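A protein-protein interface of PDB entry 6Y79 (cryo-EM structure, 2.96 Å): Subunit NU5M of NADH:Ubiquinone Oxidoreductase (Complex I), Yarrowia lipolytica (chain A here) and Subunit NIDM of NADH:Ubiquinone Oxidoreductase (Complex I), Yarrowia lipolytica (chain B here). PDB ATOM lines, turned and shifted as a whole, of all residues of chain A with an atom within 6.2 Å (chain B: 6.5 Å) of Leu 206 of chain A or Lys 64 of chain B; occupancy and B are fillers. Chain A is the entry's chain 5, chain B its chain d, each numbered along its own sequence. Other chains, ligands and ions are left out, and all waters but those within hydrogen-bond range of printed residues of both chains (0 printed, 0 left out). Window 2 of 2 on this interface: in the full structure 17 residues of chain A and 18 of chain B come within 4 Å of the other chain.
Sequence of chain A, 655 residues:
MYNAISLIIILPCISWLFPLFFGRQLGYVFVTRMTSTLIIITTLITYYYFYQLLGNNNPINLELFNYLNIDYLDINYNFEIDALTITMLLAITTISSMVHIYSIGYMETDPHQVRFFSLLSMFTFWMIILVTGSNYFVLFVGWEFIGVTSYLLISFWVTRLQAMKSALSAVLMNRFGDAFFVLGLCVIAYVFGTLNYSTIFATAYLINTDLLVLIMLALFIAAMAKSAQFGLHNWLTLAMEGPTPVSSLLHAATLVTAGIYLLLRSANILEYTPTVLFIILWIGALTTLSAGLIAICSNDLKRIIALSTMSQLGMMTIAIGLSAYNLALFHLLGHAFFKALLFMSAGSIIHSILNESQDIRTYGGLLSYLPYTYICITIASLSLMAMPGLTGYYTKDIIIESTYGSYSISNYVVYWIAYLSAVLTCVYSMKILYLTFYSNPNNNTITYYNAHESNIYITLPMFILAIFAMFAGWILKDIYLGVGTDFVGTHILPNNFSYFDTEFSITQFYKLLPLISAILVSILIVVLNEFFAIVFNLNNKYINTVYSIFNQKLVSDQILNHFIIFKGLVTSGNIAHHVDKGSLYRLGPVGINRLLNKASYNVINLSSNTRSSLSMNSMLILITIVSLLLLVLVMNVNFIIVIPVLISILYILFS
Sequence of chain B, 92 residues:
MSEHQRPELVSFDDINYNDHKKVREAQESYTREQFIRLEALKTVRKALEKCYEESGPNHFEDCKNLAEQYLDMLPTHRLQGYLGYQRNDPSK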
ATOM      1  N   ALA A 202     -20.677  -1.701   3.973  1.00  0.00           N
ATOM      2  CA  ALA A 202     -21.358  -0.767   4.859  1.00  0.00           C
ATOM      3  C   ALA A 202     -20.444   0.371   5.289  1.00  0.00           C
ATOM      4  O   ALA A 202     -20.923   1.473   5.571  1.00  0.00           O
ATOM      5  CB  ALA A 202     -21.893  -1.505   6.084  1.00  0.00           C
ATOM      6  N   THR A 203     -19.135   0.132   5.341  1.00  0.00           N
ATOM      7  CA  THR A 203     -18.173   1.107   5.834  1.00  0.00           C
ATOM      8  C   THR A 203     -17.206   1.578   4.760  1.00  0.00           C
ATOM      9  O   THR A 203     -16.164   2.144   5.090  1.00  0.00           O
ATOM     10  CB  THR A 203     -17.378   0.527   7.002  1.00  0.00           C
ATOM     11  OG1 THR A 203     -16.747  -0.691   6.594  1.00  0.00           O
ATOM     12  CG2 THR A 203     -18.274   0.250   8.172  1.00  0.00           C
ATOM     13  N   ALA A 204     -17.516   1.355   3.485  1.00  0.00           N
ATOM     14  CA  ALA A 204     -16.547   1.654   2.437  1.00  0.00           C
ATOM     15  C   ALA A 204     -16.436   3.142   2.151  1.00  0.00           C
ATOM     16  O   ALA A 204     -15.342   3.627   1.856  1.00  0.00           O
ATOM     17  CB  ALA A 204     -16.907   0.922   1.147  1.00  0.00           C
ATOM     18  N   TYR A 205     -17.542   3.878   2.235  1.00  0.00           N
ATOM     19  CA  TYR A 205     -17.554   5.294   1.892  1.00  0.00           C
ATOM     20  C   TYR A 205     -16.834   6.163   2.912  1.00  0.00           C
ATOM     21  O   TYR A 205     -16.542   7.325   2.615  1.00  0.00           O
ATOM     22  CB  TYR A 205     -18.994   5.793   1.714  1.00  0.00           C
ATOM     23  CG  TYR A 205     -19.887   5.765   2.939  1.00  0.00           C
ATOM     24  CD1 TYR A 205     -20.442   4.576   3.395  1.00  0.00           C
ATOM     25  CD2 TYR A 205     -20.218   6.935   3.605  1.00  0.00           C
ATOM     26  CE1 TYR A 205     -21.264   4.548   4.500  1.00  0.00           C
ATOM     27  CE2 TYR A 205     -21.048   6.918   4.707  1.00  0.00           C
ATOM     28  CZ  TYR A 205     -21.564   5.720   5.152  1.00  0.00           C
ATOM     29  OH  TYR A 205     -22.389   5.689   6.251  1.00  0.00           O
ATOM     30  N   LEU A 206     -16.534   5.633   4.091  1.00  0.00           N
ATOM     31  CA  LEU A 206     -15.847   6.398   5.112  1.00  0.00           C
ATOM     32  C   LEU A 206     -14.336   6.314   5.011  1.00  0.00           C
ATOM     33  O   LEU A 206     -13.665   7.275   5.379  1.00  0.00           O
ATOM     34  CB  LEU A 206     -16.300   5.928   6.491  1.00  0.00           C
ATOM     35  CG  LEU A 206     -17.802   6.140   6.628  1.00  0.00           C
ATOM     36  CD1 LEU A 206     -18.350   5.522   7.899  1.00  0.00           C
ATOM     37  CD2 LEU A 206     -18.088   7.625   6.568  1.00  0.00           C
ATOM     38  N   ILE A 207     -13.800   5.213   4.481  1.00  0.00           N
ATOM     39  CA  ILE A 207     -12.365   4.937   4.489  1.00  0.00           C
ATOM     40  C   ILE A 207     -11.627   5.906   3.566  1.00  0.00           C
ATOM     41  O   ILE A 207     -12.183   6.402   2.579  1.00  0.00           O
ATOM     42  CB  ILE A 207     -12.171   3.461   4.090  1.00  0.00           C
ATOM     43  CG1 ILE A 207     -12.921   2.575   5.075  1.00  0.00           C
ATOM     44  CG2 ILE A 207     -10.716   3.013   4.068  1.00  0.00           C
ATOM     45  CD1 ILE A 207     -12.422   2.683   6.483  1.00  0.00           C
ATOM     46  N   ASN A 208     -10.381   6.229   3.940  1.00  0.00           N
ATOM     47  CA  ASN A 208      -9.513   7.110   3.170  1.00  0.00           C
ATOM     48  C   ASN A 208      -9.294   6.594   1.756  1.00  0.00           C
ATOM     49  O   ASN A 208      -9.296   5.388   1.506  1.00  0.00           O
ATOM     50  CB  ASN A 208      -8.164   7.258   3.871  1.00  0.00           C
ATOM     51  CG  ASN A 208      -7.359   8.429   3.344  1.00  0.00           C
ATOM     52  OD1 ASN A 208      -7.838   9.216   2.530  1.00  0.00           O
ATOM     53  ND2 ASN A 208      -6.128   8.546   3.797  1.00  0.00           N
ATOM     54  N   CYS B  51     -27.816  -4.021  10.078  1.00  0.00           N
ATOM     55  CA  CYS B  51     -28.312  -2.744   9.555  1.00  0.00           C
ATOM     56  C   CYS B  51     -28.185  -2.663   8.042  1.00  0.00           C
ATOM     57  O   CYS B  51     -29.130  -2.277   7.349  1.00  0.00           O
ATOM     58  CB  CYS B  51     -27.560  -1.558  10.156  1.00  0.00           C
ATOM     59  SG  CYS B  51     -27.947  -0.048   9.199  1.00  0.00           S
ATOM     60  N   HIS B  59     -28.578   2.651   3.572  1.00  0.00           N
ATOM     61  CA  HIS B  59     -27.646   2.307   4.643  1.00  0.00           C
ATOM     62  C   HIS B  59     -26.632   3.399   4.914  1.00  0.00           C
ATOM     63  O   HIS B  59     -25.984   3.386   5.967  1.00  0.00           O
ATOM     64  CB  HIS B  59     -26.911   1.021   4.293  1.00  0.00           C
ATOM     65  CG  HIS B  59     -26.000   1.146   3.113  1.00  0.00           C
ATOM     66  ND1 HIS B  59     -24.656   1.432   3.225  1.00  0.00           N
ATOM     67  CD2 HIS B  59     -26.254   1.046   1.790  1.00  0.00           C
ATOM     68  CE1 HIS B  59     -24.121   1.491   2.020  1.00  0.00           C
ATOM     69  NE2 HIS B  59     -25.070   1.259   1.133  1.00  0.00           N
ATOM     70  N   PHE B  60     -26.457   4.312   3.965  1.00  0.00           N
ATOM     71  CA  PHE B  60     -25.647   5.495   4.200  1.00  0.00           C
ATOM     72  C   PHE B  60     -26.210   6.346   5.335  1.00  0.00           C
ATOM     73  O   PHE B  60     -25.453   6.850   6.169  1.00  0.00           O
ATOM     74  CB  PHE B  60     -25.558   6.290   2.908  1.00  0.00           C
ATOM     75  CG  PHE B  60     -24.904   5.549   1.802  1.00  0.00           C
ATOM     76  CD1 PHE B  60     -23.535   5.396   1.787  1.00  0.00           C
ATOM     77  CD2 PHE B  60     -25.655   4.983   0.786  1.00  0.00           C
ATOM     78  CE1 PHE B  60     -22.922   4.702   0.778  1.00  0.00           C
ATOM     79  CE2 PHE B  60     -25.042   4.288  -0.232  1.00  0.00           C
ATOM     80  CZ  PHE B  60     -23.672   4.149  -0.236  1.00  0.00           C
ATOM     81  N   GLU B  61     -27.532   6.466   5.434  1.00  0.00           N
ATOM     82  CA  GLU B  61     -28.064   7.370   6.448  1.00  0.00           C
ATOM     83  C   GLU B  61     -28.761   6.678   7.605  1.00  0.00           C
ATOM     84  O   GLU B  61     -28.985   7.334   8.626  1.00  0.00           O
ATOM     85  CB  GLU B  61     -29.053   8.339   5.830  1.00  0.00           C
ATOM     86  CG  GLU B  61     -29.987   7.552   5.047  1.00  0.00           C
ATOM     87  CD  GLU B  61     -30.940   8.390   4.203  1.00  0.00           C
ATOM     88  OE1 GLU B  61     -31.528   7.786   3.296  1.00  0.00           O
ATOM     89  OE2 GLU B  61     -31.077   9.577   4.507  1.00  0.00           O
ATOM     90  N   ASP B  62     -29.175   5.413   7.466  1.00  0.00           N
ATOM     91  CA  ASP B  62     -29.713   4.724   8.631  1.00  0.00           C
ATOM     92  C   ASP B  62     -28.602   4.420   9.615  1.00  0.00           C
ATOM     93  O   ASP B  62     -28.737   4.720  10.796  1.00  0.00           O
ATOM     94  CB  ASP B  62     -30.452   3.441   8.234  1.00  0.00           C
ATOM     95  CG  ASP B  62     -31.286   2.836   9.396  1.00  0.00           C
ATOM     96  OD1 ASP B  62     -30.777   2.568  10.522  1.00  0.00           O
ATOM     97  OD2 ASP B  62     -32.503   2.655   9.198  1.00  0.00           O
ATOM     98  N   CYS B  63     -27.493   3.858   9.160  1.00  0.00           N
ATOM     99  CA  CYS B  63     -26.415   3.531  10.081  1.00  0.00           C
ATOM    100  C   CYS B  63     -25.115   4.187   9.646  1.00  0.00           C
ATOM    101  O   CYS B  63     -24.091   3.537   9.437  1.00  0.00           O
ATOM    102  CB  CYS B  63     -26.270   2.030  10.297  1.00  0.00           C
ATOM    103  SG  CYS B  63     -26.184   0.941   8.895  1.00  0.00           S
ATOM    104  N   LYS B  64     -25.165   5.503   9.458  1.00  0.00           N
ATOM    105  CA  LYS B  64     -23.929   6.269   9.523  1.00  0.00           C
ATOM    106  C   LYS B  64     -23.277   6.123  10.891  1.00  0.00           C
ATOM    107  O   LYS B  64     -22.074   5.866  10.977  1.00  0.00           O
ATOM    108  CB  LYS B  64     -24.167   7.746   9.209  1.00  0.00           C
ATOM    109  CG  LYS B  64     -22.864   8.501   9.029  1.00  0.00           C
ATOM    110  CD  LYS B  64     -23.084   9.914   8.563  1.00  0.00           C
ATOM    111  CE  LYS B  64     -21.781  10.690   8.564  1.00  0.00           C
ATOM    112  NZ  LYS B  64     -20.813  10.162   7.572  1.00  0.00           N
ATOM    113  N   ASN B  65     -24.061   6.218  11.970  1.00  0.00           N
ATOM    114  CA  ASN B  65     -23.467   6.219  13.306  1.00  0.00           C
ATOM    115  C   ASN B  65     -22.944   4.842  13.704  1.00  0.00           C
ATOM    116  O   ASN B  65     -21.928   4.751  14.396  1.00  0.00           O
ATOM    117  CB  ASN B  65     -24.467   6.724  14.345  1.00  0.00           C
ATOM    118  CG  ASN B  65     -24.737   8.209  14.227  1.00  0.00           C
ATOM    119  OD1 ASN B  65     -23.818   9.005  14.047  1.00  0.00           O
ATOM    120  ND2 ASN B  65     -26.003   8.592  14.340  1.00  0.00           N
ATOM    121  N   LEU B  66     -23.592   3.761  13.257  1.00  0.00           N
ATOM    122  CA  LEU B  66     -23.059   2.424  13.522  1.00  0.00           C
ATOM    123  C   LEU B  66     -21.756   2.182  12.770  1.00  0.00           C
ATOM    124  O   LEU B  66     -20.829   1.563  13.303  1.00  0.00           O
ATOM    125  CB  LEU B  66     -24.077   1.353  13.145  1.00  0.00           C
ATOM    126  CG  LEU B  66     -25.209   1.036  14.111  1.00  0.00           C
ATOM    127  CD1 LEU B  66     -26.131   0.000  13.506  1.00  0.00           C
ATOM    128  CD2 LEU B  66     -24.648   0.539  15.417  1.00  0.00           C
ATOM    129  N   ALA B  67     -21.664   2.682  11.537  1.00  0.00           N
ATOM    130  CA  ALA B  67     -20.445   2.522  10.755  1.00  0.00           C
ATOM    131  C   ALA B  67     -19.303   3.346  11.335  1.00  0.00           C
ATOM    132  O   ALA B  67     -18.166   2.863  11.425  1.00  0.00           O
ATOM    133  CB  ALA B  67     -20.708   2.911   9.304  1.00  0.00           C
ATOM    134  N   GLU B  68     -19.595   4.587  11.740  1.00  0.00           N
ATOM    135  CA  GLU B  68     -18.609   5.413  12.426  1.00  0.00           C
ATOM    136  C   GLU B  68     -18.189   4.803  13.751  1.00  0.00           C
ATOM    137  O   GLU B  68     -17.015   4.885  14.117  1.00  0.00           O
ATOM    138  CB  GLU B  68     -19.153   6.820  12.671  1.00  0.00           C
ATOM    139  CG  GLU B  68     -19.466   7.625  11.431  1.00  0.00           C
ATOM    140  CD  GLU B  68     -18.302   8.434  10.937  1.00  0.00           C
ATOM    141  OE1 GLU B  68     -17.618   9.068  11.758  1.00  0.00           O
ATOM    142  OE2 GLU B  68     -18.070   8.446   9.718  1.00  0.00           O
ATOM    143  N   GLN B  69     -19.119   4.168  14.467  1.00  0.00           N
ATOM    144  CA  GLN B  69     -18.784   3.543  15.737  1.00  0.00           C
ATOM    145  C   GLN B  69     -17.857   2.353  15.541  1.00  0.00           C
ATOM    146  O   GLN B  69     -16.879   2.194  16.281  1.00  0.00           O
ATOM    147  CB  GLN B  69     -20.055   3.114  16.456  1.00  0.00           C
ATOM    148  CG  GLN B  69     -19.783   2.321  17.701  1.00  0.00           C
ATOM    149  CD  GLN B  69     -21.027   1.802  18.334  1.00  0.00           C
ATOM    150  OE1 GLN B  69     -22.080   1.778  17.709  1.00  0.00           O
ATOM    151  NE2 GLN B  69     -20.920   1.363  19.577  1.00  0.00           N
ATOM    152  N   LEU B  71     -15.820   1.842  12.966  1.00  0.00           N
ATOM    153  CA  LEU B  71     -14.502   2.240  12.497  1.00  0.00           C
ATOM    154  C   LEU B  71     -13.766   3.124  13.496  1.00  0.00           C
ATOM    155  O   LEU B  71     -12.569   3.365  13.319  1.00  0.00           O
ATOM    156  CB  LEU B  71     -14.619   2.937  11.152  1.00  0.00           C
ATOM    157  CG  LEU B  71     -15.072   2.131   9.944  1.00  0.00           C
ATOM    158  CD1 LEU B  71     -15.315   3.093   8.804  1.00  0.00           C
ATOM    159  CD2 LEU B  71     -14.039   1.078   9.573  1.00  0.00           C
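Of the 7 printed residues of chain A, 4 touch a printed residue of chain B.
Hydrophobic or aromatic side chains of chain A that line the printed part of chain B: Tyr 205, Leu 206 and Ile 207.
Hydrophobic or aromatic side chains of chain B within 4 Å of the printed part of chain A: Phe 60, Ala 67 and Leu 71.
Along chain B the printed residues that touch a printed residue of chain A span positions 60 to 71.
Among the printed residues, 9 pairs touch across the chains.
Among the printed residues, no Asp or Glu carboxylate lies within 4 Å of a Lys or Arg side-chain nitrogen of the other chain.
CB of Ala 67 of chain B touches CG2 of Thr 203 of chain A (3.8 Å).
Thr 203 of chain A touches Leu 71 of chain B (CB to CD1, 3.8 Å).
Lys 64 of chain B touches Tyr 205 of chain A (CA to OH, 3.7 Å).
CD2 of Leu 206 of chain A touches NZ of Lys 64 of chain B, 3.9 Å away.
Leu 206 of chain A touches Ala 67 of chain B.
Glu 68 of chain B touches Leu 206 of chain A (OE2 to CD2, 3.3 Å).
CB of Leu 206 of chain A touches CD1 of Leu 71 of chain B (3.8 Å).
CD1 of Ile 207 of chain A touches CD1 of Leu 71 of chain B, 3.7 Å away.
Printed residues of chain A within 4 Å of Lys 64 of chain B: Tyr 205 and Leu 206.
Of the printed residues of chain A, Glu 68 of chain B touches Leu 206 (3.3 Å).
Of the printed residues of chain A, Leu 71 of chain B touches Thr 203 (3.8 Å), Leu 206 (3.8 Å) and Ile 207 (3.7 Å).
The nearest residue of chain B that does not touch Leu 206 of chain A is Cys 63 of chain B (6.3 Å).
The nearest printed residue of chain A that does not touch Lys 64 of chain B is Ala 202 of chain A (6.9 Å).
The nearest printed residue of chain A that does not touch Phe 60 of chain B is Ala 202 of chain A (6.0 Å).
The side-chain amino group (NZ) of Lys 64 of chain B is in salt-bridge range of the side-chain carboxylate (OE2) of Glu 68 of chain B (3.9 Å).
The side-chain sulfur of Cys 51 of chain B is disulfide-bonded to the side-chain sulfur of Cys 63 of chain B (2.0 Å).
OH of Tyr 205 of chain A is in hydrogen-bond range of O of Phe 60 of chain B (3.3 Å).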
